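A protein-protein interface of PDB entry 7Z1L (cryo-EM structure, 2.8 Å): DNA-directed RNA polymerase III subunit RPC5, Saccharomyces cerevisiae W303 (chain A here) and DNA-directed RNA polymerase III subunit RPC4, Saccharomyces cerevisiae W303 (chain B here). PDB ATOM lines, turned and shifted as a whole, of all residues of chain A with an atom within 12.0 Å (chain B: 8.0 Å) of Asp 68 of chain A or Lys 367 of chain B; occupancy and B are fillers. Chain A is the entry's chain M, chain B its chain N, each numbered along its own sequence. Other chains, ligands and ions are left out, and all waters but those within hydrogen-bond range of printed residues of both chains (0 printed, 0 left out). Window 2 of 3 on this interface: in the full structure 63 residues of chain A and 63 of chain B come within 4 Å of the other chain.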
ATOM      1  N   ASP A  68      23.689   5.880 -19.432  1.00  0.00           N
ATOM      2  CA  ASP A  68      23.588   7.174 -18.759  1.00  0.00           C
ATOM      3  C   ASP A  68      24.177   8.363 -19.558  1.00  0.00           C
ATOM      4  O   ASP A  68      23.588   9.444 -19.530  1.00  0.00           O
ATOM      5  CB  ASP A  68      24.234   7.099 -17.366  1.00  0.00           C
ATOM      6  CG  ASP A  68      23.837   5.850 -16.606  1.00  0.00           C
ATOM      7  OD1 ASP A  68      22.716   5.347 -16.830  1.00  0.00           O
ATOM      8  OD2 ASP A  68      24.646   5.371 -15.785  1.00  0.00           O
ATOM      9  N   PRO A  69      25.318   8.204 -20.249  1.00  0.00           N
ATOM     10  CA  PRO A  69      25.736   9.264 -21.176  1.00  0.00           C
ATOM     11  C   PRO A  69      24.749   9.441 -22.320  1.00  0.00           C
ATOM     12  O   PRO A  69      24.064   8.504 -22.736  1.00  0.00           O
ATOM     13  CB  PRO A  69      27.098   8.779 -21.684  1.00  0.00           C
ATOM     14  CG  PRO A  69      27.621   7.960 -20.589  1.00  0.00           C
ATOM     15  CD  PRO A  69      26.429   7.252 -20.025  1.00  0.00           C
ATOM     16  N   VAL A  70      24.685  10.666 -22.824  1.00  0.00           N
ATOM     17  CA  VAL A  70      23.780  11.034 -23.906  1.00  0.00           C
ATOM     18  C   VAL A  70      24.508  10.909 -25.235  1.00  0.00           C
ATOM     19  O   VAL A  70      25.643  11.377 -25.387  1.00  0.00           O
ATOM     20  CB  VAL A  70      23.244  12.462 -23.701  1.00  0.00           C
ATOM     21  CG1 VAL A  70      22.183  12.780 -24.734  1.00  0.00           C
ATOM     22  CG2 VAL A  70      22.695  12.622 -22.293  1.00  0.00           C
ATOM     23  N   ILE A  71      23.856  10.274 -26.208  1.00  0.00           N
ATOM     24  CA  ILE A  71      24.458  10.123 -27.527  1.00  0.00           C
ATOM     25  C   ILE A  71      24.098  11.276 -28.462  1.00  0.00           C
ATOM     26  O   ILE A  71      24.899  11.635 -29.332  1.00  0.00           O
ATOM     27  CB  ILE A  71      24.070   8.766 -28.143  1.00  0.00           C
ATOM     28  CG1 ILE A  71      22.553   8.644 -28.297  1.00  0.00           C
ATOM     29  CG2 ILE A  71      24.607   7.627 -27.296  1.00  0.00           C
ATOM     30  CD1 ILE A  71      22.118   7.455 -29.125  1.00  0.00           C
ATOM     31  N   GLU A  72      22.918  11.874 -28.304  1.00  0.00           N
ATOM     32  CA  GLU A  72      22.502  12.982 -29.150  1.00  0.00           C
ATOM     33  C   GLU A  72      21.442  13.797 -28.425  1.00  0.00           C
ATOM     34  O   GLU A  72      20.660  13.269 -27.629  1.00  0.00           O
ATOM     35  CB  GLU A  72      21.973  12.496 -30.506  1.00  0.00           C
ATOM     36  CG  GLU A  72      20.746  11.604 -30.421  1.00  0.00           C
ATOM     37  CD  GLU A  72      20.169  11.278 -31.785  1.00  0.00           C
ATOM     38  OE1 GLU A  72      20.490  11.997 -32.753  1.00  0.00           O
ATOM     39  OE2 GLU A  72      19.395  10.302 -31.887  1.00  0.00           O
ATOM     40  N   GLU A  73      21.425  15.097 -28.710  1.00  0.00           N
ATOM     41  CA  GLU A  73      20.484  16.015 -28.088  1.00  0.00           C
ATOM     42  C   GLU A  73      19.776  16.829 -29.160  1.00  0.00           C
ATOM     43  O   GLU A  73      20.405  17.296 -30.112  1.00  0.00           O
ATOM     44  CB  GLU A  73      21.185  16.963 -27.105  1.00  0.00           C
ATOM     45  CG  GLU A  73      22.002  16.266 -26.035  1.00  0.00           C
ATOM     46  CD  GLU A  73      22.465  17.214 -24.948  1.00  0.00           C
ATOM     47  OE1 GLU A  73      22.060  18.395 -24.977  1.00  0.00           O
ATOM     48  OE2 GLU A  73      23.232  16.777 -24.064  1.00  0.00           O
ATOM     49  N   PHE A  74      18.466  16.992 -28.996  1.00  0.00           N
ATOM     50  CA  PHE A  74      17.676  17.851 -29.870  1.00  0.00           C
ATOM     51  C   PHE A  74      17.308  19.116 -29.110  1.00  0.00           C
ATOM     52  O   PHE A  74      16.551  19.038 -28.128  1.00  0.00           O
ATOM     53  CB  PHE A  74      16.414  17.136 -30.357  1.00  0.00           C
ATOM     54  CG  PHE A  74      16.668  15.776 -30.949  1.00  0.00           C
ATOM     55  CD1 PHE A  74      17.797  15.533 -31.716  1.00  0.00           C
ATOM     56  CD2 PHE A  74      15.772  14.743 -30.740  1.00  0.00           C
ATOM     57  CE1 PHE A  74      18.027  14.283 -32.258  1.00  0.00           C
ATOM     58  CE2 PHE A  74      15.996  13.491 -31.279  1.00  0.00           C
ATOM     59  CZ  PHE A  74      17.125  13.261 -32.039  1.00  0.00           C
ATOM     60  N   GLN B 288      10.715   5.036 -27.906  1.00  0.00           N
ATOM     61  CA  GLN B 288      11.170   4.705 -29.256  1.00  0.00           C
ATOM     62  C   GLN B 288      10.250   5.303 -30.317  1.00  0.00           C
ATOM     63  O   GLN B 288      10.721   5.825 -31.340  1.00  0.00           O
ATOM     64  CB  GLN B 288      11.268   3.188 -29.419  1.00  0.00           C
ATOM     65  CG  GLN B 288      12.293   2.543 -28.506  1.00  0.00           C
ATOM     66  CD  GLN B 288      12.782   1.209 -29.029  1.00  0.00           C
ATOM     67  OE1 GLN B 288      12.182   0.626 -29.933  1.00  0.00           O
ATOM     68  NE2 GLN B 288      13.877   0.717 -28.463  1.00  0.00           N
ATOM     69  N   ARG B 364      16.985  14.604 -24.961  1.00  0.00           N
ATOM     70  CA  ARG B 364      18.180  13.779 -24.933  1.00  0.00           C
ATOM     71  C   ARG B 364      17.809  12.312 -25.083  1.00  0.00           C
ATOM     72  O   ARG B 364      16.817  11.850 -24.507  1.00  0.00           O
ATOM     73  CB  ARG B 364      18.942  13.982 -23.624  1.00  0.00           C
ATOM     74  CG  ARG B 364      18.995  15.418 -23.144  1.00  0.00           C
ATOM     75  CD  ARG B 364      20.046  15.576 -22.065  1.00  0.00           C
ATOM     76  NE  ARG B 364      20.007  14.466 -21.122  1.00  0.00           N
ATOM     77  CZ  ARG B 364      19.671  14.580 -19.846  1.00  0.00           C
ATOM     78  NH1 ARG B 364      19.353  15.750 -19.317  1.00  0.00           N
ATOM     79  NH2 ARG B 364      19.655  13.493 -19.079  1.00  0.00           N
ATOM     80  N   VAL B 365      18.622  11.586 -25.846  1.00  0.00           N
ATOM     81  CA  VAL B 365      18.452  10.158 -26.078  1.00  0.00           C
ATOM     82  C   VAL B 365      19.655   9.438 -25.486  1.00  0.00           C
ATOM     83  O   VAL B 365      20.801   9.821 -25.746  1.00  0.00           O
ATOM     84  CB  VAL B 365      18.311   9.840 -27.578  1.00  0.00           C
ATOM     85  CG1 VAL B 365      18.030   8.359 -27.785  1.00  0.00           C
ATOM     86  CG2 VAL B 365      17.218  10.691 -28.201  1.00  0.00           C
ATOM     87  N   HIS B 366      19.395   8.406 -24.692  1.00  0.00           N
ATOM     88  CA  HIS B 366      20.444   7.617 -24.066  1.00  0.00           C
ATOM     89  C   HIS B 366      20.655   6.313 -24.830  1.00  0.00           C
ATOM     90  O   HIS B 366      19.920   5.981 -25.762  1.00  0.00           O
ATOM     91  CB  HIS B 366      20.101   7.339 -22.601  1.00  0.00           C
ATOM     92  CG  HIS B 366      19.795   8.572 -21.809  1.00  0.00           C
ATOM     93  ND1 HIS B 366      18.539   9.137 -21.767  1.00  0.00           N
ATOM     94  CD2 HIS B 366      20.584   9.351 -21.031  1.00  0.00           C
ATOM     95  CE1 HIS B 366      18.566  10.209 -20.995  1.00  0.00           C
ATOM     96  NE2 HIS B 366      19.795  10.362 -20.536  1.00  0.00           N
ATOM     97  N   LYS B 367      21.690   5.571 -24.421  1.00  0.00           N
ATOM     98  CA  LYS B 367      22.017   4.318 -25.098  1.00  0.00           C
ATOM     99  C   LYS B 367      20.946   3.259 -24.878  1.00  0.00           C
ATOM    100  O   LYS B 367      20.766   2.375 -25.723  1.00  0.00           O
ATOM    101  CB  LYS B 367      23.375   3.800 -24.628  1.00  0.00           C
ATOM    102  CG  LYS B 367      24.542   4.697 -24.994  1.00  0.00           C
ATOM    103  CD  LYS B 367      25.719   4.469 -24.064  1.00  0.00           C
ATOM    104  CE  LYS B 367      25.377   4.893 -22.649  1.00  0.00           C
ATOM    105  NZ  LYS B 367      24.662   6.197 -22.632  1.00  0.00           N
ATOM    106  N   SER B 368      20.228   3.326 -23.756  1.00  0.00           N
ATOM    107  CA  SER B 368      19.130   2.402 -23.510  1.00  0.00           C
ATOM    108  C   SER B 368      17.900   2.714 -24.351  1.00  0.00           C
ATOM    109  O   SER B 368      16.959   1.912 -24.361  1.00  0.00           O
ATOM    110  CB  SER B 368      18.756   2.410 -22.028  1.00  0.00           C
ATOM    111  OG  SER B 368      18.064   3.598 -21.685  1.00  0.00           O
ATOM    112  N   GLY B 369      17.883   3.847 -25.052  1.00  0.00           N
ATOM    113  CA  GLY B 369      16.745   4.253 -25.841  1.00  0.00           C
ATOM    114  C   GLY B 369      15.766   5.161 -25.132  1.00  0.00           C
ATOM    115  O   GLY B 369      14.832   5.658 -25.774  1.00  0.00           O
ATOM    116  N   LYS B 370      15.944   5.392 -23.834  1.00  0.00           N
ATOM    117  CA  LYS B 370      15.047   6.277 -23.106  1.00  0.00           C
ATOM    118  C   LYS B 370      15.301   7.729 -23.491  1.00  0.00           C
ATOM    119  O   LYS B 370      16.425   8.120 -23.812  1.00  0.00           O
ATOM    120  CB  LYS B 370      15.218   6.082 -21.598  1.00  0.00           C
ATOM    121  CG  LYS B 370      16.579   6.481 -21.055  1.00  0.00           C
ATOM    122  CD  LYS B 370      16.747   6.045 -19.608  1.00  0.00           C
ATOM    123  CE  LYS B 370      15.850   6.846 -18.682  1.00  0.00           C
ATOM    124  NZ  LYS B 370      16.250   8.278 -18.623  1.00  0.00           N
ATOM    125  N   SER B 372      14.737  11.885 -22.431  1.00  0.00           N
ATOM    126  CA  SER B 372      14.569  12.765 -21.283  1.00  0.00           C
ATOM    127  C   SER B 372      14.636  14.213 -21.738  1.00  0.00           C
ATOM    128  O   SER B 372      15.516  14.577 -22.519  1.00  0.00           O
ATOM    129  CB  SER B 372      15.640  12.496 -20.221  1.00  0.00           C
ATOM    130  OG  SER B 372      16.808  13.256 -20.476  1.00  0.00           O
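Asp 68 of chain A touches His 366 of chain B. O of Pro 69 of chain A touches CA of His 366 of chain B (3.96 Å). Val 70 of chain A touches Arg 364 of chain B. Val 70 of chain A touches Val 365 of chain B (CG1 to O, 3.4 Å). Ile 71 of chain A touches Lys 367 of chain B. CA of Arg 364 of chain B touches O of Glu 72 of chain A, 3.7 Å away. Arg 364 of chain B touches Glu 73 of chain A.
Of chain B, only His 366 and Lys 367 come within 4 Å of Asp 68 of chain A. Lys 367 of chain B touches just these residues of chain A: Asp 68, Pro 69 and Ile 71. Val 365 of chain B touches just these residues of chain A: Val 70, Ile 71 and Glu 72. No residue of chain A comes within 4 Å of Ser 368 of chain B. No residue of chain A comes within 4 Å of Gly 369 of chain B. No residue of chain A comes within 4 Å of Lys 370 of chain B. Of the printed residues of chain B, Val 70 of chain A touches Arg 364 and Val 365. Printed residues of chain A within 4 Å of Arg 364 of chain B: Val 70 (3.5 Å), Glu 72 (3.7 Å) and Glu 73 (3.9 Å). Printed residues of chain B within 4 Å of Glu 72 of chain A: Arg 364 and Val 365. Of the printed residues of chain B, Ile 71 of chain A touches Val 365 and Lys 367. Printed residues of chain B within 4 Å of Glu 73 of chain A: Arg 364. The nearest printed residue of chain B that does not touch Ile 71 of chain A is His 366 of chain B (4.3 Å).
The backbone carbonyl oxygen (O) of Val 365 of chain B is in hydrogen-bond range of the backbone NH (N) of Ile 71 of chain A (3.1 Å). O of Glu 72 of chain A sits at hydrogen-bond distance from N of Val 365 of chain B, 3.2 Å away. The side-chain amino group (NZ) of Lys 367 of chain B lies close to the backbone NH (N) of Asp 68 of chain A (3.4 Å). The backbone carbonyl oxygen (O) of Pro 69 of chain A lies close to the side-chain amino group (NZ) of Lys 367 of chain B (2.4 Å).
NE2 of His 366 of chain B lies within hydrogen-bond range of NH2 of Arg 364 of chain B (3.5 Å). N of Arg 364 of chain B sits at hydrogen-bond distance from O of Ser 372 of chain B, at 2.8 Å. ND1 of His 366 of chain B lies within hydrogen-bond range of O of Lys 370 of chain B (3.1 Å).
Of the 9 printed residues of chain B, 4 touch a printed residue of chain A. Printed residues of chain B that touch a printed residue of chain A: Arg 364, Val 365, His 366 and Lys 367. Of the 7 printed residues of chain A, 6 touch a printed residue of chain B. Among the printed residues, no Asp or Glu carboxylate lies within 4 Å of a Lys or Arg side-chain nitrogen of the other chain.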
